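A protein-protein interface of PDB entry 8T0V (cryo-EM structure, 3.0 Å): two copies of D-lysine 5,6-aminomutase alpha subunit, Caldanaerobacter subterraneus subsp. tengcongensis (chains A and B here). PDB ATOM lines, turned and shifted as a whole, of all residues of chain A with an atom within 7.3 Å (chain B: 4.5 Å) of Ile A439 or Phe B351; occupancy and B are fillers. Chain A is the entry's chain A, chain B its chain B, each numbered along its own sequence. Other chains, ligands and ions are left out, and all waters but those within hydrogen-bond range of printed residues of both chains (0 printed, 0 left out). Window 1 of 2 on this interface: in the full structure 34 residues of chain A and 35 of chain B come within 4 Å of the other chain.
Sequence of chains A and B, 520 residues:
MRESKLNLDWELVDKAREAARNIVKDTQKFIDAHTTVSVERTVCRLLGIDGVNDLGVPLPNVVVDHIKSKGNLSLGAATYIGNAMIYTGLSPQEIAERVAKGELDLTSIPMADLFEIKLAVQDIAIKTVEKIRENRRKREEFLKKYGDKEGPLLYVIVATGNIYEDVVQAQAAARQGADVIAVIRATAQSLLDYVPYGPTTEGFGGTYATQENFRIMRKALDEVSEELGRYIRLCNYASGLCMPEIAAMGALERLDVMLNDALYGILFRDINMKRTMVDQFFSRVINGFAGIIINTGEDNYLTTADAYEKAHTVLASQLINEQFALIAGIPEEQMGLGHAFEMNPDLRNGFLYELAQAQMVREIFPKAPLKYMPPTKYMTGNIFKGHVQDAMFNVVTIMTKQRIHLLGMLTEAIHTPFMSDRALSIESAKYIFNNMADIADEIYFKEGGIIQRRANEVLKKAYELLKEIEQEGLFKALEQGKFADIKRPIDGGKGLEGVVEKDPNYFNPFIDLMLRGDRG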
ATOM      1  N   LYS A   5     -41.692 -22.714 -33.318  1.00  0.00           N
ATOM      2  CA  LYS A   5     -40.459 -23.393 -33.691  1.00  0.00           C
ATOM      3  C   LYS A   5     -40.560 -24.902 -33.557  1.00  0.00           C
ATOM      4  O   LYS A   5     -39.773 -25.615 -34.185  1.00  0.00           O
ATOM      5  CB  LYS A   5     -39.298 -22.904 -32.828  1.00  0.00           C
ATOM      6  CG  LYS A   5     -38.679 -21.609 -33.280  1.00  0.00           C
ATOM      7  CD  LYS A   5     -37.318 -21.436 -32.652  1.00  0.00           C
ATOM      8  CE  LYS A   5     -36.666 -20.144 -33.075  1.00  0.00           C
ATOM      9  NZ  LYS A   5     -35.383 -19.948 -32.368  1.00  0.00           N
ATOM     10  N   VAL A 395     -26.946 -21.141 -20.979  1.00  0.00           N
ATOM     11  CA  VAL A 395     -27.055 -21.313 -22.424  1.00  0.00           C
ATOM     12  C   VAL A 395     -28.500 -21.590 -22.810  1.00  0.00           C
ATOM     13  O   VAL A 395     -29.034 -21.013 -23.765  1.00  0.00           O
ATOM     14  CB  VAL A 395     -26.118 -22.443 -22.889  1.00  0.00           C
ATOM     15  CG1 VAL A 395     -26.500 -22.930 -24.269  1.00  0.00           C
ATOM     16  CG2 VAL A 395     -24.679 -21.973 -22.866  1.00  0.00           C
ATOM     17  N   ILE A 398     -30.654 -18.330 -22.416  1.00  0.00           N
ATOM     18  CA  ILE A 398     -30.499 -17.348 -23.486  1.00  0.00           C
ATOM     19  C   ILE A 398     -31.087 -17.873 -24.788  1.00  0.00           C
ATOM     20  O   ILE A 398     -31.681 -17.115 -25.562  1.00  0.00           O
ATOM     21  CB  ILE A 398     -29.022 -16.940 -23.652  1.00  0.00           C
ATOM     22  CG1 ILE A 398     -28.902 -15.751 -24.603  1.00  0.00           C
ATOM     23  CG2 ILE A 398     -28.192 -18.086 -24.173  1.00  0.00           C
ATOM     24  CD1 ILE A 398     -29.491 -14.474 -24.069  1.00  0.00           C
ATOM     25  N   MET A 399     -30.938 -19.171 -25.058  1.00  0.00           N
ATOM     26  CA  MET A 399     -31.391 -19.709 -26.332  1.00  0.00           C
ATOM     27  C   MET A 399     -32.903 -19.852 -26.413  1.00  0.00           C
ATOM     28  O   MET A 399     -33.435 -19.955 -27.522  1.00  0.00           O
ATOM     29  CB  MET A 399     -30.730 -21.064 -26.588  1.00  0.00           C
ATOM     30  CG  MET A 399     -30.684 -21.450 -28.057  1.00  0.00           C
ATOM     31  SD  MET A 399     -29.862 -23.019 -28.417  1.00  0.00           S
ATOM     32  CE  MET A 399     -28.510 -23.010 -27.251  1.00  0.00           C
ATOM     33  N   THR A 400     -33.609 -19.869 -25.280  1.00  0.00           N
ATOM     34  CA  THR A 400     -35.066 -19.992 -25.284  1.00  0.00           C
ATOM     35  C   THR A 400     -35.787 -18.727 -24.833  1.00  0.00           C
ATOM     36  O   THR A 400     -37.019 -18.695 -24.862  1.00  0.00           O
ATOM     37  CB  THR A 400     -35.503 -21.156 -24.394  1.00  0.00           C
ATOM     38  OG1 THR A 400     -35.131 -20.890 -23.039  1.00  0.00           O
ATOM     39  CG2 THR A 400     -34.842 -22.435 -24.843  1.00  0.00           C
ATOM     40  N   LYS A 401     -35.060 -17.687 -24.425  1.00  0.00           N
ATOM     41  CA  LYS A 401     -35.657 -16.407 -24.059  1.00  0.00           C
ATOM     42  C   LYS A 401     -36.534 -16.493 -22.817  1.00  0.00           C
ATOM     43  O   LYS A 401     -37.724 -16.166 -22.871  1.00  0.00           O
ATOM     44  CB  LYS A 401     -36.481 -15.859 -25.223  1.00  0.00           C
ATOM     45  CG  LYS A 401     -35.771 -15.911 -26.551  1.00  0.00           C
ATOM     46  CD  LYS A 401     -36.497 -15.090 -27.598  1.00  0.00           C
ATOM     47  CE  LYS A 401     -35.932 -13.687 -27.701  1.00  0.00           C
ATOM     48  NZ  LYS A 401     -36.259 -13.068 -29.012  1.00  0.00           N
ATOM     49  N   TYR A 431     -21.304 -13.196 -19.173  1.00  0.00           N
ATOM     50  CA  TYR A 431     -20.518 -13.615 -20.328  1.00  0.00           C
ATOM     51  C   TYR A 431     -21.386 -14.360 -21.335  1.00  0.00           C
ATOM     52  O   TYR A 431     -21.405 -14.036 -22.531  1.00  0.00           O
ATOM     53  CB  TYR A 431     -19.354 -14.485 -19.851  1.00  0.00           C
ATOM     54  CG  TYR A 431     -18.701 -15.328 -20.923  1.00  0.00           C
ATOM     55  CD1 TYR A 431     -18.112 -14.742 -22.030  1.00  0.00           C
ATOM     56  CD2 TYR A 431     -18.655 -16.709 -20.817  1.00  0.00           C
ATOM     57  CE1 TYR A 431     -17.511 -15.507 -23.004  1.00  0.00           C
ATOM     58  CE2 TYR A 431     -18.057 -17.478 -21.789  1.00  0.00           C
ATOM     59  CZ  TYR A 431     -17.487 -16.871 -22.877  1.00  0.00           C
ATOM     60  OH  TYR A 431     -16.887 -17.632 -23.847  1.00  0.00           O
ATOM     61  N   ILE A 432     -22.133 -15.356 -20.857  1.00  0.00           N
ATOM     62  CA  ILE A 432     -22.909 -16.194 -21.767  1.00  0.00           C
ATOM     63  C   ILE A 432     -24.052 -15.402 -22.388  1.00  0.00           C
ATOM     64  O   ILE A 432     -24.401 -15.608 -23.554  1.00  0.00           O
ATOM     65  CB  ILE A 432     -23.411 -17.451 -21.038  1.00  0.00           C
ATOM     66  CG1 ILE A 432     -22.228 -18.352 -20.690  1.00  0.00           C
ATOM     67  CG2 ILE A 432     -24.392 -18.204 -21.902  1.00  0.00           C
ATOM     68  CD1 ILE A 432     -22.507 -19.334 -19.602  1.00  0.00           C
ATOM     69  N   ASN A 434     -24.071 -12.190 -23.033  1.00  0.00           N
ATOM     70  CA  ASN A 434     -23.533 -11.246 -24.006  1.00  0.00           C
ATOM     71  C   ASN A 434     -23.117 -11.950 -25.290  1.00  0.00           C
ATOM     72  O   ASN A 434     -23.449 -11.496 -26.390  1.00  0.00           O
ATOM     73  CB  ASN A 434     -22.351 -10.493 -23.400  1.00  0.00           C
ATOM     74  CG  ASN A 434     -21.820  -9.412 -24.310  1.00  0.00           C
ATOM     75  OD1 ASN A 434     -22.584  -8.712 -24.971  1.00  0.00           O
ATOM     76  ND2 ASN A 434     -20.505  -9.261 -24.343  1.00  0.00           N
ATOM     77  N   ASN A 435     -22.395 -13.068 -25.176  1.00  0.00           N
ATOM     78  CA  ASN A 435     -21.841 -13.710 -26.367  1.00  0.00           C
ATOM     79  C   ASN A 435     -22.934 -14.233 -27.290  1.00  0.00           C
ATOM     80  O   ASN A 435     -22.849 -14.086 -28.511  1.00  0.00           O
ATOM     81  CB  ASN A 435     -20.905 -14.844 -25.967  1.00  0.00           C
ATOM     82  CG  ASN A 435     -19.487 -14.384 -25.800  1.00  0.00           C
ATOM     83  OD1 ASN A 435     -18.607 -14.735 -26.585  1.00  0.00           O
ATOM     84  ND2 ASN A 435     -19.252 -13.585 -24.777  1.00  0.00           N
ATOM     85  N   MET A 436     -23.962 -14.859 -26.726  1.00  0.00           N
ATOM     86  CA  MET A 436     -25.018 -15.509 -27.497  1.00  0.00           C
ATOM     87  C   MET A 436     -26.289 -14.676 -27.522  1.00  0.00           C
ATOM     88  O   MET A 436     -27.394 -15.215 -27.497  1.00  0.00           O
ATOM     89  CB  MET A 436     -25.301 -16.893 -26.926  1.00  0.00           C
ATOM     90  CG  MET A 436     -24.093 -17.572 -26.294  1.00  0.00           C
ATOM     91  SD  MET A 436     -24.442 -19.175 -25.547  1.00  0.00           S
ATOM     92  CE  MET A 436     -25.448 -19.954 -26.793  1.00  0.00           C
ATOM     93  N   ALA A 437     -26.156 -13.351 -27.592  1.00  0.00           N
ATOM     94  CA  ALA A 437     -27.302 -12.473 -27.387  1.00  0.00           C
ATOM     95  C   ALA A 437     -28.423 -12.773 -28.373  1.00  0.00           C
ATOM     96  O   ALA A 437     -29.578 -12.959 -27.975  1.00  0.00           O
ATOM     97  CB  ALA A 437     -26.862 -11.017 -27.499  1.00  0.00           C
ATOM     98  N   ASP A 438     -28.108 -12.824 -29.667  1.00  0.00           N
ATOM     99  CA  ASP A 438     -29.112 -13.010 -30.708  1.00  0.00           C
ATOM    100  C   ASP A 438     -29.175 -14.447 -31.209  1.00  0.00           C
ATOM    101  O   ASP A 438     -29.570 -14.683 -32.353  1.00  0.00           O
ATOM    102  CB  ASP A 438     -28.848 -12.061 -31.876  1.00  0.00           C
ATOM    103  CG  ASP A 438     -29.129 -10.615 -31.528  1.00  0.00           C
ATOM    104  OD1 ASP A 438     -30.168 -10.342 -30.895  1.00  0.00           O
ATOM    105  OD2 ASP A 438     -28.314  -9.745 -31.893  1.00  0.00           O
ATOM    106  N   ILE A 439     -28.791 -15.416 -30.375  1.00  0.00           N
ATOM    107  CA  ILE A 439     -28.847 -16.812 -30.797  1.00  0.00           C
ATOM    108  C   ILE A 439     -30.285 -17.295 -30.902  1.00  0.00           C
ATOM    109  O   ILE A 439     -30.593 -18.167 -31.720  1.00  0.00           O
ATOM    110  CB  ILE A 439     -28.030 -17.699 -29.843  1.00  0.00           C
ATOM    111  CG1 ILE A 439     -27.811 -19.071 -30.481  1.00  0.00           C
ATOM    112  CG2 ILE A 439     -28.723 -17.824 -28.509  1.00  0.00           C
ATOM    113  CD1 ILE A 439     -26.669 -19.852 -29.890  1.00  0.00           C
ATOM    114  N   ALA A 440     -31.184 -16.756 -30.081  1.00  0.00           N
ATOM    115  CA  ALA A 440     -32.576 -17.179 -30.142  1.00  0.00           C
ATOM    116  C   ALA A 440     -33.178 -16.888 -31.507  1.00  0.00           C
ATOM    117  O   ALA A 440     -33.973 -17.677 -32.022  1.00  0.00           O
ATOM    118  CB  ALA A 440     -33.379 -16.486 -29.046  1.00  0.00           C
ATOM    119  N   ASP A 441     -32.812 -15.756 -32.107  1.00  0.00           N
ATOM    120  CA  ASP A 441     -33.363 -15.374 -33.400  1.00  0.00           C
ATOM    121  C   ASP A 441     -32.793 -16.191 -34.548  1.00  0.00           C
ATOM    122  O   ASP A 441     -33.406 -16.236 -35.619  1.00  0.00           O
ATOM    123  CB  ASP A 441     -33.097 -13.891 -33.669  1.00  0.00           C
ATOM    124  CG  ASP A 441     -33.695 -12.982 -32.609  1.00  0.00           C
ATOM    125  OD1 ASP A 441     -34.250 -13.491 -31.616  1.00  0.00           O
ATOM    126  OD2 ASP A 441     -33.608 -11.750 -32.771  1.00  0.00           O
ATOM    127  N   GLU A 442     -31.645 -16.836 -34.350  1.00  0.00           N
ATOM    128  CA  GLU A 442     -30.932 -17.514 -35.430  1.00  0.00           C
ATOM    129  C   GLU A 442     -31.275 -18.998 -35.506  1.00  0.00           C
ATOM    130  O   GLU A 442     -31.769 -19.474 -36.531  1.00  0.00           O
ATOM    131  CB  GLU A 442     -29.422 -17.334 -35.244  1.00  0.00           C
ATOM    132  CG  GLU A 442     -28.944 -15.897 -35.340  1.00  0.00           C
ATOM    133  CD  GLU A 442     -29.157 -15.300 -36.714  1.00  0.00           C
ATOM    134  OE1 GLU A 442     -28.637 -15.869 -37.695  1.00  0.00           O
ATOM    135  OE2 GLU A 442     -29.841 -14.260 -36.814  1.00  0.00           O
ATOM    136  N   ILE A 443     -31.026 -19.738 -34.427  1.00  0.00           N
ATOM    137  CA  ILE A 443     -31.110 -21.194 -34.473  1.00  0.00           C
ATOM    138  C   ILE A 443     -32.568 -21.625 -34.560  1.00  0.00           C
ATOM    139  O   ILE A 443     -33.396 -21.245 -33.727  1.00  0.00           O
ATOM    140  CB  ILE A 443     -30.425 -21.825 -33.255  1.00  0.00           C
ATOM    141  CG1 ILE A 443     -31.045 -21.304 -31.958  1.00  0.00           C
ATOM    142  CG2 ILE A 443     -28.933 -21.554 -33.285  1.00  0.00           C
ATOM    143  CD1 ILE A 443     -31.843 -22.339 -31.217  1.00  0.00           C
ATOM    144  N   TYR A 444     -32.881 -22.421 -35.577  1.00  0.00           N
ATOM    145  CA  TYR A 444     -34.149 -23.105 -35.732  1.00  0.00           C
ATOM    146  C   TYR A 444     -33.954 -24.568 -35.350  1.00  0.00           C
ATOM    147  O   TYR A 444     -32.909 -24.956 -34.828  1.00  0.00           O
ATOM    148  CB  TYR A 444     -34.659 -22.956 -37.163  1.00  0.00           C
ATOM    149  CG  TYR A 444     -35.073 -21.557 -37.551  1.00  0.00           C
ATOM    150  CD1 TYR A 444     -35.041 -20.513 -36.637  1.00  0.00           C
ATOM    151  CD2 TYR A 444     -35.494 -21.280 -38.841  1.00  0.00           C
ATOM    152  CE1 TYR A 444     -35.425 -19.236 -36.995  1.00  0.00           C
ATOM    153  CE2 TYR A 444     -35.878 -20.006 -39.209  1.00  0.00           C
ATOM    154  CZ  TYR A 444     -35.840 -18.990 -38.282  1.00  0.00           C
ATOM    155  OH  TYR A 444     -36.222 -17.724 -38.652  1.00  0.00           O
ATOM    156  N   ASN B 349     -22.308 -11.278 -29.604  1.00  0.00           N
ATOM    157  CA  ASN B 349     -22.511 -12.185 -30.729  1.00  0.00           C
ATOM    158  C   ASN B 349     -21.210 -12.816 -31.203  1.00  0.00           C
ATOM    159  O   ASN B 349     -21.104 -13.221 -32.358  1.00  0.00           O
ATOM    160  CB  ASN B 349     -23.199 -11.483 -31.903  1.00  0.00           C
ATOM    161  CG  ASN B 349     -24.645 -11.165 -31.624  1.00  0.00           C
ATOM    162  OD1 ASN B 349     -25.215 -11.634 -30.645  1.00  0.00           O
ATOM    163  ND2 ASN B 349     -25.252 -10.374 -32.495  1.00  0.00           N
ATOM    164  N   GLY B 350     -20.203 -12.903 -30.335  1.00  0.00           N
ATOM    165  CA  GLY B 350     -18.970 -13.572 -30.718  1.00  0.00           C
ATOM    166  C   GLY B 350     -19.169 -15.057 -30.940  1.00  0.00           C
ATOM    167  O   GLY B 350     -18.522 -15.662 -31.799  1.00  0.00           O
ATOM    168  N   PHE B 351     -20.058 -15.668 -30.157  1.00  0.00           N
ATOM    169  CA  PHE B 351     -20.355 -17.083 -30.331  1.00  0.00           C
ATOM    170  C   PHE B 351     -20.945 -17.351 -31.706  1.00  0.00           C
ATOM    171  O   PHE B 351     -20.631 -18.363 -32.336  1.00  0.00           O
ATOM    172  CB  PHE B 351     -21.307 -17.547 -29.228  1.00  0.00           C
ATOM    173  CG  PHE B 351     -21.533 -19.028 -29.200  1.00  0.00           C
ATOM    174  CD1 PHE B 351     -20.668 -19.860 -28.519  1.00  0.00           C
ATOM    175  CD2 PHE B 351     -22.618 -19.588 -29.843  1.00  0.00           C
ATOM    176  CE1 PHE B 351     -20.878 -21.218 -28.490  1.00  0.00           C
ATOM    177  CE2 PHE B 351     -22.827 -20.947 -29.816  1.00  0.00           C
ATOM    178  CZ  PHE B 351     -21.958 -21.759 -29.137  1.00  0.00           C
ATOM    179  N   LEU B 352     -21.804 -16.455 -32.194  1.00  0.00           N
ATOM    180  CA  LEU B 352     -22.382 -16.643 -33.519  1.00  0.00           C
ATOM    181  C   LEU B 352     -21.313 -16.557 -34.600  1.00  0.00           C
ATOM    182  O   LEU B 352     -21.354 -17.301 -35.584  1.00  0.00           O
ATOM    183  CB  LEU B 352     -23.484 -15.614 -33.769  1.00  0.00           C
ATOM    184  CG  LEU B 352     -24.510 -15.355 -32.660  1.00  0.00           C
ATOM    185  CD1 LEU B 352     -25.763 -14.767 -33.269  1.00  0.00           C
ATOM    186  CD2 LEU B 352     -24.841 -16.593 -31.862  1.00  0.00           C
ATOM    187  N   TYR B 353     -20.340 -15.660 -34.434  1.00  0.00           N
ATOM    188  CA  TYR B 353     -19.260 -15.538 -35.410  1.00  0.00           C
ATOM    189  C   TYR B 353     -18.374 -16.775 -35.414  1.00  0.00           C
ATOM    190  O   TYR B 353     -18.019 -17.296 -36.478  1.00  0.00           O
ATOM    191  CB  TYR B 353     -18.436 -14.289 -35.112  1.00  0.00           C
ATOM    192  CG  TYR B 353     -19.243 -13.014 -35.171  1.00  0.00           C
ATOM    193  CD1 TYR B 353     -20.283 -12.872 -36.075  1.00  0.00           C
ATOM    194  CD2 TYR B 353     -18.962 -11.955 -34.329  1.00  0.00           C
ATOM    195  CE1 TYR B 353     -21.021 -11.721 -36.134  1.00  0.00           C
ATOM    196  CE2 TYR B 353     -19.694 -10.796 -34.382  1.00  0.00           C
ATOM    197  CZ  TYR B 353     -20.722 -10.684 -35.289  1.00  0.00           C
ATOM    198  OH  TYR B 353     -21.460  -9.528 -35.349  1.00  0.00           O
ATOM    199  N   GLU B 354     -18.005 -17.266 -34.232  1.00  0.00           N
ATOM    200  CA  GLU B 354     -17.201 -18.481 -34.170  1.00  0.00           C
ATOM    201  C   GLU B 354     -17.959 -19.673 -34.742  1.00  0.00           C
ATOM    202  O   GLU B 354     -17.385 -20.509 -35.447  1.00  0.00           O
ATOM    203  CB  GLU B 354     -16.766 -18.744 -32.733  1.00  0.00           C
ATOM    204  CG  GLU B 354     -15.509 -17.985 -32.373  1.00  0.00           C
ATOM    205  CD  GLU B 354     -15.545 -17.387 -30.990  1.00  0.00           C
ATOM    206  OE1 GLU B 354     -16.645 -17.246 -30.425  1.00  0.00           O
ATOM    207  OE2 GLU B 354     -14.469 -17.032 -30.472  1.00  0.00           O
ATOM    208  N   LEU B 355     -19.255 -19.770 -34.448  1.00  0.00           N
ATOM    209  CA  LEU B 355     -20.066 -20.857 -34.981  1.00  0.00           C
ATOM    210  C   LEU B 355     -20.148 -20.786 -36.501  1.00  0.00           C
ATOM    211  O   LEU B 355     -20.030 -21.806 -37.189  1.00  0.00           O
ATOM    212  CB  LEU B 355     -21.458 -20.798 -34.351  1.00  0.00           C
ATOM    213  CG  LEU B 355     -22.442 -21.950 -34.552  1.00  0.00           C
ATOM    214  CD1 LEU B 355     -21.925 -23.221 -33.913  1.00  0.00           C
ATOM    215  CD2 LEU B 355     -23.789 -21.572 -33.971  1.00  0.00           C
ATOM    216  N   MET B 392     -17.727 -23.374 -23.563  1.00  0.00           N
ATOM    217  CA  MET B 392     -18.259 -22.817 -24.807  1.00  0.00           C
ATOM    218  C   MET B 392     -17.490 -23.338 -26.017  1.00  0.00           C
ATOM    219  O   MET B 392     -18.067 -23.571 -27.088  1.00  0.00           O
ATOM    220  CB  MET B 392     -18.224 -21.292 -24.758  1.00  0.00           C
ATOM    221  CG  MET B 392     -18.915 -20.698 -23.540  1.00  0.00           C
ATOM    222  SD  MET B 392     -20.586 -21.322 -23.285  1.00  0.00           S
ATOM    223  CE  MET B 392     -21.446 -20.568 -24.655  1.00  0.00           C
ATOM    224  N   VAL B 395     -18.826 -26.640 -26.731  1.00  0.00           N
ATOM    225  CA  VAL B 395     -20.162 -26.490 -27.304  1.00  0.00           C
ATOM    226  C   VAL B 395     -20.065 -26.254 -28.804  1.00  0.00           C
ATOM    227  O   VAL B 395     -20.799 -26.855 -29.597  1.00  0.00           O
ATOM    228  CB  VAL B 395     -20.916 -25.349 -26.600  1.00  0.00           C
ATOM    229  CG1 VAL B 395     -22.232 -25.067 -27.297  1.00  0.00           C
ATOM    230  CG2 VAL B 395     -21.139 -25.686 -25.141  1.00  0.00           C
ATOM    231  N   VAL B 396     -19.154 -25.372 -29.218  1.00  0.00           N
ATOM    232  CA  VAL B 396     -18.977 -25.111 -30.646  1.00  0.00           C
ATOM    233  C   VAL B 396     -18.443 -26.352 -31.351  1.00  0.00           C
ATOM    234  O   VAL B 396     -18.794 -26.632 -32.502  1.00  0.00           O
ATOM    235  CB  VAL B 396     -18.050 -23.904 -30.870  1.00  0.00           C
ATOM    236  CG1 VAL B 396     -17.794 -23.715 -32.347  1.00  0.00           C
ATOM    237  CG2 VAL B 396     -18.650 -22.659 -30.279  1.00  0.00           C
ATOM    238  N   MET B 399     -21.478 -28.754 -31.717  1.00  0.00           N
ATOM    239  CA  MET B 399     -22.549 -28.260 -32.575  1.00  0.00           C
ATOM    240  C   MET B 399     -22.146 -28.311 -34.042  1.00  0.00           C
ATOM    241  O   MET B 399     -22.959 -28.665 -34.901  1.00  0.00           O
ATOM    242  CB  MET B 399     -22.925 -26.841 -32.159  1.00  0.00           C
ATOM    243  CG  MET B 399     -24.277 -26.388 -32.682  1.00  0.00           C
ATOM    244  SD  MET B 399     -24.966 -24.885 -31.949  1.00  0.00           S
ATOM    245  CE  MET B 399     -23.952 -24.636 -30.500  1.00  0.00           C
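The backbone carbonyl oxygen of Asn A435 sits at hydrogen-bond distance from the backbone NH of Gly B350 (3.4 Å).
The backbone NH of Asn B349 sits at hydrogen-bond distance from the backbone carbonyl oxygen of Asn A434, at 3.4 Å.
ND2 of Asn B349 is in hydrogen-bond range of OD2 of Asp A438, 3.2 Å away.
N of Asn B349 lies close to O of Asn A435 (3.1 Å).
ND2 of Asn A435 lies close to O of Tyr A431 (3.1 Å).
Among the printed residues, pairs that only touch across the chains: Val A395 with Met B392 (3.95 Å), Tyr A431 with Met B392 (3.7 Å), Asn A435 with Phe B351 (3.6 Å), Met A436 with Met B392 (3.4 Å), Ala A437 with Asn B349 (3.6 Å), Asp A438 with Leu B352 (3.9 Å), Ile A439 with Phe B351 (3.996 Å), Ile A439 with Leu B352 (3.9 Å) and Glu A442 with Leu B352 (3.96 Å).
Printed residues of chain B within 4 Å of Asn A434: Asn B349.
Of the printed residues of chain B, Asp A438 touches Asn B349 and Leu B352.
Printed residues of chain B within 4 Å of Ile A439: Phe B351 (3.996 Å) and Leu B352 (3.9 Å).
Gly B350 touches one residue of chain A.
Of the printed residues of chain A, Phe B351 touches Asn A435 and Ile A439.
Of the printed residues of chain A, Met B392 touches Val A395, Tyr A431 and Met A436.
The nearest printed residue of chain A that does not touch Phe B351 is Met A436 (4.05 Å).
The nearest printed residue of chain A that does not touch Leu B352 is Met A436 (4.5 Å).
Of the 19 printed residues of chain A, 9 touch a printed residue of chain B.
Hydrophobic or aromatic side chains of chain A that line the printed part of chain B: Val A395, Tyr A431, Met A436, Ala A437 and Ile A439.
Printed residues of chain B that touch a printed residue of chain A: Asn B349, Gly B350, Phe B351, Leu B352 and Met B392.
Hydrophobic or aromatic side chains of chain B that line the printed part of chain A: Phe B351, Leu B352 and Met B392.
Among the printed residues, 13 pairs touch across the chains.
Among the printed residues, no Asp or Glu carboxylate lies within 4 Å of a Lys or Arg side-chain nitrogen of the other chain.
Positions printed for both chains: 395 and 399.
Of the 13 pairs that touch across the chains among the printed residues, none has its exchanged pair printed and touching as well.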
